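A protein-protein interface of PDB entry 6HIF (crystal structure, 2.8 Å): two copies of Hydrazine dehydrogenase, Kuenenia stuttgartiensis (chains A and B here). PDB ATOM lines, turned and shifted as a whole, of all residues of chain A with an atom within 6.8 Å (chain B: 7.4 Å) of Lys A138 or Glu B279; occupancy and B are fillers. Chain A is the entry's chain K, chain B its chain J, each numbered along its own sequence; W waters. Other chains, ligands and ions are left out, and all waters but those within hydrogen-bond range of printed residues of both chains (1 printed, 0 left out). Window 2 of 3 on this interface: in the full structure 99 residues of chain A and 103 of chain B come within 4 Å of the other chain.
The side-chain amino group of Lys A138 sits at hydrogen-bond distance from the backbone carbonyl oxygen of Glu B279 (3.1 Å).
The side-chain amide nitrogen (NE2) of Gln B280 lies close to the side-chain amide nitrogen (NE2) of Gln A235.
OD2 of Asp A135 is in hydrogen-bond range of N of His A234, at 3.4 Å.
N of Glu B279 sits at hydrogen-bond distance from OD1 of Asp B277 (3.0 Å).
The side-chain carboxylate of Asp A135 lies close to the side-chain amide oxygen of Gln A235, at 3.0 Å.
The side-chain amino group (NZ) of Lys B285 lies within salt-bridge range of the side-chain carboxylate (OD1) of Asp B291 (3.2 Å).
The backbone NH (N) of Val B293 is in hydrogen-bond range of the backbone carbonyl oxygen (O) of Gln B280.
NE of Arg A134 touches O of Asp B291 (3.6 Å).
Asp A135 touches Val B293.
CD of Lys A138 touches NE2 of Gln B280, 3.9 Å away.
OE1 of Gln A235 touches CG2 of Val B293, at 3.5 Å.
Of the printed residues of chain B, Asp A135 touches Val B293.
Lys A138 touches two residues of chain B.
Printed residues of chain B within 4 Å of Gln A235: Gln B280 (3.0 Å) and Val B293 (3.5 Å).
Of chain A, only Lys A138 comes within 4 Å of Glu B279.
Of the printed residues of chain A, Gln B280 touches Lys A138 and Gln A235.
Printed residues of chain A within 4 Å of Val B293: Asp A135 (3.6 Å) and Gln A235 (3.5 Å).
The nearest printed residue of chain B that does not touch Gln A235 is Asn B274 (5.4 Å).
Printed residues of chain B that touch a printed residue of chain A: Glu B279, Gln B280, Asp B291 and Val B293.
Hydrophobic or aromatic side chains of chain B that line the printed part of chain A: Val B293.
Among the printed residues, 6 pairs touch across the chains.
Among the printed residues, no Asp or Glu carboxylate lies within 4 Å of a Lys or Arg side-chain nitrogen of the other chain.
No position is printed for both chains.
Of the 6 pairs that touch across the chains among the printed residues, none has its exchanged pair printed and touching as well.
Water W1 bridges O of Tyr B292 (2.7 Å) and NE of Arg A134 (3.3 Å).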
ATOM      1  N   VAL A 133      12.590  -0.941  16.587  1.00  0.00           N
ATOM      2  CA  VAL A 133      12.414  -0.911  18.031  1.00  0.00           C
ATOM      3  C   VAL A 133      12.805  -2.263  18.622  1.00  0.00           C
ATOM      4  O   VAL A 133      13.461  -2.296  19.664  1.00  0.00           O
ATOM      5  CB  VAL A 133      10.993  -0.469  18.435  1.00  0.00           C
ATOM      6  CG1 VAL A 133      10.681  -0.787  19.892  1.00  0.00           C
ATOM      7  CG2 VAL A 133      10.777   1.010  18.155  1.00  0.00           C
ATOM      8  N   ARG A 134      12.420  -3.361  17.944  1.00  0.00           N
ATOM      9  CA  ARG A 134      12.812  -4.704  18.353  1.00  0.00           C
ATOM     10  C   ARG A 134      14.331  -4.797  18.469  1.00  0.00           C
ATOM     11  O   ARG A 134      14.834  -5.343  19.448  1.00  0.00           O
ATOM     12  CB  ARG A 134      12.292  -5.772  17.388  1.00  0.00           C
ATOM     13  CG  ARG A 134      11.163  -6.622  17.953  1.00  0.00           C
ATOM     14  CD  ARG A 134      10.825  -7.833  17.100  1.00  0.00           C
ATOM     15  NE  ARG A 134      10.551  -7.499  15.707  1.00  0.00           N
ATOM     16  CZ  ARG A 134       9.381  -7.081  15.241  1.00  0.00           C
ATOM     17  NH1 ARG A 134       8.337  -6.989  16.047  1.00  0.00           N
ATOM     18  NH2 ARG A 134       9.260  -6.751  13.968  1.00  0.00           N
ATOM     19  N   ASP A 135      15.041  -4.254  17.469  1.00  0.00           N
ATOM     20  CA  ASP A 135      16.494  -4.247  17.431  1.00  0.00           C
ATOM     21  C   ASP A 135      17.050  -3.377  18.556  1.00  0.00           C
ATOM     22  O   ASP A 135      17.975  -3.783  19.258  1.00  0.00           O
ATOM     23  CB  ASP A 135      17.010  -3.781  16.068  1.00  0.00           C
ATOM     24  CG  ASP A 135      16.930  -4.855  14.996  1.00  0.00           C
ATOM     25  OD1 ASP A 135      16.509  -5.984  15.322  1.00  0.00           O
ATOM     26  OD2 ASP A 135      17.293  -4.556  13.843  1.00  0.00           O
ATOM     27  N   TYR A 136      16.466  -2.181  18.715  1.00  0.00           N
ATOM     28  CA  TYR A 136      16.926  -1.206  19.691  1.00  0.00           C
ATOM     29  C   TYR A 136      16.854  -1.799  21.097  1.00  0.00           C
ATOM     30  O   TYR A 136      17.795  -1.666  21.876  1.00  0.00           O
ATOM     31  CB  TYR A 136      16.142   0.106  19.574  1.00  0.00           C
ATOM     32  CG  TYR A 136      16.341   1.044  20.738  1.00  0.00           C
ATOM     33  CD1 TYR A 136      17.507   1.784  20.874  1.00  0.00           C
ATOM     34  CD2 TYR A 136      15.375   1.163  21.727  1.00  0.00           C
ATOM     35  CE1 TYR A 136      17.700   2.630  21.955  1.00  0.00           C
ATOM     36  CE2 TYR A 136      15.552   2.007  22.813  1.00  0.00           C
ATOM     37  CZ  TYR A 136      16.718   2.744  22.926  1.00  0.00           C
ATOM     38  OH  TYR A 136      16.903   3.575  23.990  1.00  0.00           O
ATOM     39  N   ASN A 137      15.731  -2.459  21.402  1.00  0.00           N
ATOM     40  CA  ASN A 137      15.481  -2.993  22.732  1.00  0.00           C
ATOM     41  C   ASN A 137      16.485  -4.093  23.062  1.00  0.00           C
ATOM     42  O   ASN A 137      16.814  -4.288  24.227  1.00  0.00           O
ATOM     43  CB  ASN A 137      14.036  -3.462  22.904  1.00  0.00           C
ATOM     44  CG  ASN A 137      13.049  -2.316  22.951  1.00  0.00           C
ATOM     45  OD1 ASN A 137      13.394  -1.200  23.337  1.00  0.00           O
ATOM     46  ND2 ASN A 137      11.813  -2.577  22.561  1.00  0.00           N
ATOM     47  N   LYS A 138      16.970  -4.793  22.028  1.00  0.00           N
ATOM     48  CA  LYS A 138      17.952  -5.851  22.202  1.00  0.00           C
ATOM     49  C   LYS A 138      19.333  -5.243  22.435  1.00  0.00           C
ATOM     50  O   LYS A 138      20.178  -5.869  23.060  1.00  0.00           O
ATOM     51  CB  LYS A 138      17.979  -6.785  20.987  1.00  0.00           C
ATOM     52  CG  LYS A 138      16.825  -7.774  20.865  1.00  0.00           C
ATOM     53  CD  LYS A 138      16.906  -8.617  19.605  1.00  0.00           C
ATOM     54  CE  LYS A 138      15.631  -9.360  19.255  1.00  0.00           C
ATOM     55  NZ  LYS A 138      15.553 -10.681  19.924  1.00  0.00           N
ATOM     56  N   SER A 139      19.547  -4.022  21.930  1.00  0.00           N
ATOM     57  CA  SER A 139      20.858  -3.391  21.925  1.00  0.00           C
ATOM     58  C   SER A 139      21.270  -2.975  23.334  1.00  0.00           C
ATOM     59  O   SER A 139      20.420  -2.730  24.187  1.00  0.00           O
ATOM     60  CB  SER A 139      20.885  -2.216  20.986  1.00  0.00           C
ATOM     61  OG  SER A 139      20.320  -1.062  21.593  1.00  0.00           O
ATOM     62  N   ALA A 140      22.588  -2.877  23.549  1.00  0.00           N
ATOM     63  CA  ALA A 140      23.148  -2.453  24.821  1.00  0.00           C
ATOM     64  C   ALA A 140      22.811  -0.986  25.076  1.00  0.00           C
ATOM     65  O   ALA A 140      22.726  -0.555  26.225  1.00  0.00           O
ATOM     66  CB  ALA A 140      24.638  -2.683  24.826  1.00  0.00           C
ATOM     67  N   HIS A 141      22.625  -0.236  23.982  1.00  0.00           N
ATOM     68  CA  HIS A 141      22.340   1.189  24.023  1.00  0.00           C
ATOM     69  C   HIS A 141      21.109   1.469  24.885  1.00  0.00           C
ATOM     70  O   HIS A 141      21.079   2.455  25.625  1.00  0.00           O
ATOM     71  CB  HIS A 141      22.158   1.736  22.598  1.00  0.00           C
ATOM     72  CG  HIS A 141      23.428   1.919  21.838  1.00  0.00           C
ATOM     73  ND1 HIS A 141      23.625   1.365  20.590  1.00  0.00           N
ATOM     74  CD2 HIS A 141      24.556   2.601  22.130  1.00  0.00           C
ATOM     75  CE1 HIS A 141      24.820   1.695  20.147  1.00  0.00           C
ATOM     76  NE2 HIS A 141      25.409   2.455  21.073  1.00  0.00           N
ATOM     77  N   SER A 142      20.103   0.592  24.777  1.00  0.00           N
ATOM     78  CA  SER A 142      18.823   0.793  25.434  1.00  0.00           C
ATOM     79  C   SER A 142      18.952   0.546  26.933  1.00  0.00           C
ATOM     80  O   SER A 142      18.212   1.128  27.723  1.00  0.00           O
ATOM     81  CB  SER A 142      17.760  -0.076  24.820  1.00  0.00           C
ATOM     82  OG  SER A 142      18.053  -1.450  25.013  1.00  0.00           O
ATOM     83  N   LYS A 143      19.910  -0.305  27.308  1.00  0.00           N
ATOM     84  CA  LYS A 143      20.044  -0.773  28.676  1.00  0.00           C
ATOM     85  C   LYS A 143      21.054   0.081  29.442  1.00  0.00           C
ATOM     86  O   LYS A 143      21.211  -0.083  30.652  1.00  0.00           O
ATOM     87  CB  LYS A 143      20.473  -2.242  28.684  1.00  0.00           C
ATOM     88  CG  LYS A 143      19.497  -3.227  28.058  1.00  0.00           C
ATOM     89  CD  LYS A 143      20.111  -4.604  27.898  1.00  0.00           C
ATOM     90  CE  LYS A 143      19.097  -5.671  27.548  1.00  0.00           C
ATOM     91  NZ  LYS A 143      18.571  -5.488  26.176  1.00  0.00           N
ATOM     92  N   HIS A 234      19.505  -1.970  14.385  1.00  0.00           N
ATOM     93  CA  HIS A 234      19.751  -1.069  15.499  1.00  0.00           C
ATOM     94  C   HIS A 234      20.209  -1.872  16.711  1.00  0.00           C
ATOM     95  O   HIS A 234      20.156  -1.383  17.840  1.00  0.00           O
ATOM     96  CB  HIS A 234      18.493  -0.237  15.789  1.00  0.00           C
ATOM     97  CG  HIS A 234      18.296   0.886  14.829  1.00  0.00           C
ATOM     98  ND1 HIS A 234      17.756   0.698  13.575  1.00  0.00           N
ATOM     99  CD2 HIS A 234      18.579   2.199  14.923  1.00  0.00           C
ATOM    100  CE1 HIS A 234      17.710   1.852  12.943  1.00  0.00           C
ATOM    101  NE2 HIS A 234      18.210   2.790  13.749  1.00  0.00           N
ATOM    102  N   GLN A 235      20.675  -3.098  16.446  1.00  0.00           N
ATOM    103  CA  GLN A 235      21.042  -4.062  17.471  1.00  0.00           C
ATOM    104  C   GLN A 235      22.483  -3.818  17.922  1.00  0.00           C
ATOM    105  O   GLN A 235      22.799  -3.960  19.102  1.00  0.00           O
ATOM    106  CB  GLN A 235      20.834  -5.472  16.921  1.00  0.00           C
ATOM    107  CG  GLN A 235      20.272  -6.443  17.943  1.00  0.00           C
ATOM    108  CD  GLN A 235      19.672  -7.670  17.299  1.00  0.00           C
ATOM    109  OE1 GLN A 235      18.845  -7.587  16.395  1.00  0.00           O
ATOM    110  NE2 GLN A 235      20.089  -8.830  17.771  1.00  0.00           N
ATOM    111  N   ASN B 274      22.357 -15.093  11.311  1.00  0.00           N
ATOM    112  CA  ASN B 274      21.396 -15.142  12.404  1.00  0.00           C
ATOM    113  C   ASN B 274      20.415 -16.310  12.276  1.00  0.00           C
ATOM    114  O   ASN B 274      19.652 -16.556  13.209  1.00  0.00           O
ATOM    115  CB  ASN B 274      20.608 -13.835  12.516  1.00  0.00           C
ATOM    116  CG  ASN B 274      21.452 -12.665  12.969  1.00  0.00           C
ATOM    117  OD1 ASN B 274      21.687 -12.491  14.159  1.00  0.00           O
ATOM    118  ND2 ASN B 274      21.893 -11.841  12.033  1.00  0.00           N
ATOM    119  N   TRP B 276      20.277 -19.470  12.422  1.00  0.00           N
ATOM    120  CA  TRP B 276      20.224 -20.578  13.362  1.00  0.00           C
ATOM    121  C   TRP B 276      20.121 -20.063  14.794  1.00  0.00           C
ATOM    122  O   TRP B 276      20.131 -20.853  15.733  1.00  0.00           O
ATOM    123  CB  TRP B 276      21.420 -21.519  13.179  1.00  0.00           C
ATOM    124  CG  TRP B 276      21.334 -22.341  11.928  1.00  0.00           C
ATOM    125  CD1 TRP B 276      22.012 -22.144  10.758  1.00  0.00           C
ATOM    126  CD2 TRP B 276      20.506 -23.498  11.716  1.00  0.00           C
ATOM    127  NE1 TRP B 276      21.667 -23.098   9.839  1.00  0.00           N
ATOM    128  CE2 TRP B 276      20.747 -23.945  10.398  1.00  0.00           C
ATOM    129  CE3 TRP B 276      19.589 -24.200  12.507  1.00  0.00           C
ATOM    130  CZ2 TRP B 276      20.107 -25.064   9.864  1.00  0.00           C
ATOM    131  CZ3 TRP B 276      18.954 -25.303  11.976  1.00  0.00           C
ATOM    132  CH2 TRP B 276      19.208 -25.725  10.671  1.00  0.00           C
ATOM    133  N   ASP B 277      20.040 -18.734  14.942  1.00  0.00           N
ATOM    134  CA  ASP B 277      19.778 -18.119  16.234  1.00  0.00           C
ATOM    135  C   ASP B 277      18.274 -17.904  16.354  1.00  0.00           C
ATOM    136  O   ASP B 277      17.693 -17.090  15.641  1.00  0.00           O
ATOM    137  CB  ASP B 277      20.603 -16.847  16.449  1.00  0.00           C
ATOM    138  CG  ASP B 277      20.350 -16.149  17.777  1.00  0.00           C
ATOM    139  OD1 ASP B 277      19.563 -16.676  18.590  1.00  0.00           O
ATOM    140  OD2 ASP B 277      20.946 -15.073  17.986  1.00  0.00           O
ATOM    141  N   THR B 278      17.667 -18.656  17.273  1.00  0.00           N
ATOM    142  CA  THR B 278      16.225 -18.731  17.421  1.00  0.00           C
ATOM    143  C   THR B 278      15.668 -17.403  17.943  1.00  0.00           C
ATOM    144  O   THR B 278      14.481 -17.123  17.791  1.00  0.00           O
ATOM    145  CB  THR B 278      15.853 -19.962  18.254  1.00  0.00           C
ATOM    146  OG1 THR B 278      14.432 -20.038  18.235  1.00  0.00           O
ATOM    147  CG2 THR B 278      16.360 -19.900  19.680  1.00  0.00           C
ATOM    148  N   GLU B 279      16.544 -16.582  18.534  1.00  0.00           N
ATOM    149  CA  GLU B 279      16.179 -15.278  19.070  1.00  0.00           C
ATOM    150  C   GLU B 279      16.053 -14.250  17.946  1.00  0.00           C
ATOM    151  O   GLU B 279      15.480 -13.182  18.149  1.00  0.00           O
ATOM    152  CB  GLU B 279      17.223 -14.802  20.083  1.00  0.00           C
ATOM    153  CG  GLU B 279      17.234 -15.598  21.378  1.00  0.00           C
ATOM    154  CD  GLU B 279      16.031 -15.357  22.275  1.00  0.00           C
ATOM    155  OE1 GLU B 279      16.126 -14.476  23.150  1.00  0.00           O
ATOM    156  OE2 GLU B 279      15.004 -16.049  22.100  1.00  0.00           O
ATOM    157  N   GLN B 280      16.606 -14.572  16.772  1.00  0.00           N
ATOM    158  CA  GLN B 280      16.626 -13.645  15.653  1.00  0.00           C
ATOM    159  C   GLN B 280      15.683 -14.140  14.559  1.00  0.00           C
ATOM    160  O   GLN B 280      15.005 -13.340  13.916  1.00  0.00           O
ATOM    161  CB  GLN B 280      18.050 -13.475  15.120  1.00  0.00           C
ATOM    162  CG  GLN B 280      19.051 -12.976  16.154  1.00  0.00           C
ATOM    163  CD  GLN B 280      18.699 -11.639  16.765  1.00  0.00           C
ATOM    164  OE1 GLN B 280      18.273 -10.702  16.094  1.00  0.00           O
ATOM    165  NE2 GLN B 280      18.892 -11.537  18.067  1.00  0.00           N
ATOM    166  N   PHE B 281      15.666 -15.463  14.351  1.00  0.00           N
ATOM    167  CA  PHE B 281      14.823 -16.098  13.353  1.00  0.00           C
ATOM    168  C   PHE B 281      14.121 -17.291  13.989  1.00  0.00           C
ATOM    169  O   PHE B 281      14.770 -18.278  14.323  1.00  0.00           O
ATOM    170  CB  PHE B 281      15.654 -16.542  12.146  1.00  0.00           C
ATOM    171  CG  PHE B 281      16.003 -15.444  11.175  1.00  0.00           C
ATOM    172  CD1 PHE B 281      15.152 -15.123  10.126  1.00  0.00           C
ATOM    173  CD2 PHE B 281      17.186 -14.730  11.309  1.00  0.00           C
ATOM    174  CE1 PHE B 281      15.474 -14.110   9.233  1.00  0.00           C
ATOM    175  CE2 PHE B 281      17.508 -13.718  10.413  1.00  0.00           C
ATOM    176  CZ  PHE B 281      16.650 -13.406   9.379  1.00  0.00           C
ATOM    177  N   ASP B 282      12.797 -17.177  14.148  1.00  0.00           N
ATOM    178  CA  ASP B 282      11.992 -18.262  14.683  1.00  0.00           C
ATOM    179  C   ASP B 282      11.106 -18.814  13.571  1.00  0.00           C
ATOM    180  O   ASP B 282      10.104 -18.203  13.208  1.00  0.00           O
ATOM    181  CB  ASP B 282      11.208 -17.805  15.919  1.00  0.00           C
ATOM    182  CG  ASP B 282      10.500 -18.926  16.666  1.00  0.00           C
ATOM    183  OD1 ASP B 282      10.647 -20.095  16.256  1.00  0.00           O
ATOM    184  OD2 ASP B 282       9.804 -18.622  17.658  1.00  0.00           O
ATOM    185  N   LYS B 285       7.223 -19.925  14.039  1.00  0.00           N
ATOM    186  CA  LYS B 285       6.179 -18.918  13.934  1.00  0.00           C
ATOM    187  C   LYS B 285       5.600 -18.947  12.523  1.00  0.00           C
ATOM    188  O   LYS B 285       6.323 -19.198  11.563  1.00  0.00           O
ATOM    189  CB  LYS B 285       6.756 -17.528  14.214  1.00  0.00           C
ATOM    190  CG  LYS B 285       7.080 -17.206  15.668  1.00  0.00           C
ATOM    191  CD  LYS B 285       7.237 -15.713  15.889  1.00  0.00           C
ATOM    192  CE  LYS B 285       7.347 -15.303  17.341  1.00  0.00           C
ATOM    193  NZ  LYS B 285       8.743 -15.400  17.826  1.00  0.00           N
ATOM    194  N   ASP B 291       8.626 -12.172  13.164  1.00  0.00           N
ATOM    195  CA  ASP B 291       9.229 -10.986  13.749  1.00  0.00           C
ATOM    196  C   ASP B 291      10.751 -11.091  13.646  1.00  0.00           C
ATOM    197  O   ASP B 291      11.458 -10.798  14.610  1.00  0.00           O
ATOM    198  CB  ASP B 291       8.757 -10.786  15.194  1.00  0.00           C
ATOM    199  CG  ASP B 291       9.152 -11.909  16.142  1.00  0.00           C
ATOM    200  OD1 ASP B 291       9.351 -13.048  15.672  1.00  0.00           O
ATOM    201  OD2 ASP B 291       9.264 -11.637  17.348  1.00  0.00           O
ATOM    202  N   TYR B 292      11.240 -11.501  12.465  1.00  0.00           N
ATOM    203  CA  TYR B 292      12.663 -11.719  12.241  1.00  0.00           C
ATOM    204  C   TYR B 292      13.420 -10.395  12.314  1.00  0.00           C
ATOM    205  O   TYR B 292      12.823  -9.325  12.194  1.00  0.00           O
ATOM    206  CB  TYR B 292      12.938 -12.332  10.865  1.00  0.00           C
ATOM    207  CG  TYR B 292      12.071 -13.488  10.441  1.00  0.00           C
ATOM    208  CD1 TYR B 292      11.774 -14.536  11.299  1.00  0.00           C
ATOM    209  CD2 TYR B 292      11.582 -13.554   9.146  1.00  0.00           C
ATOM    210  CE1 TYR B 292      10.979 -15.595  10.891  1.00  0.00           C
ATOM    211  CE2 TYR B 292      10.794 -14.612   8.718  1.00  0.00           C
ATOM    212  CZ  TYR B 292      10.488 -15.634   9.596  1.00  0.00           C
ATOM    213  OH  TYR B 292       9.711 -16.665   9.162  1.00  0.00           O
ATOM    214  N   VAL B 293      14.741 -10.486  12.498  1.00  0.00           N
ATOM    215  CA  VAL B 293      15.598  -9.313  12.480  1.00  0.00           C
ATOM    216  C   VAL B 293      15.693  -8.808  11.042  1.00  0.00           C
ATOM    217  O   VAL B 293      15.680  -7.599  10.794  1.00  0.00           O
ATOM    218  CB  VAL B 293      16.982  -9.601  13.100  1.00  0.00           C
ATOM    219  CG1 VAL B 293      17.673 -10.796  12.464  1.00  0.00           C
ATOM    220  CG2 VAL B 293      17.894  -8.383  13.095  1.00  0.00           C
HETATM  221  O   HOH W   1      13.348  -7.263  13.895  1.00  0.00           O
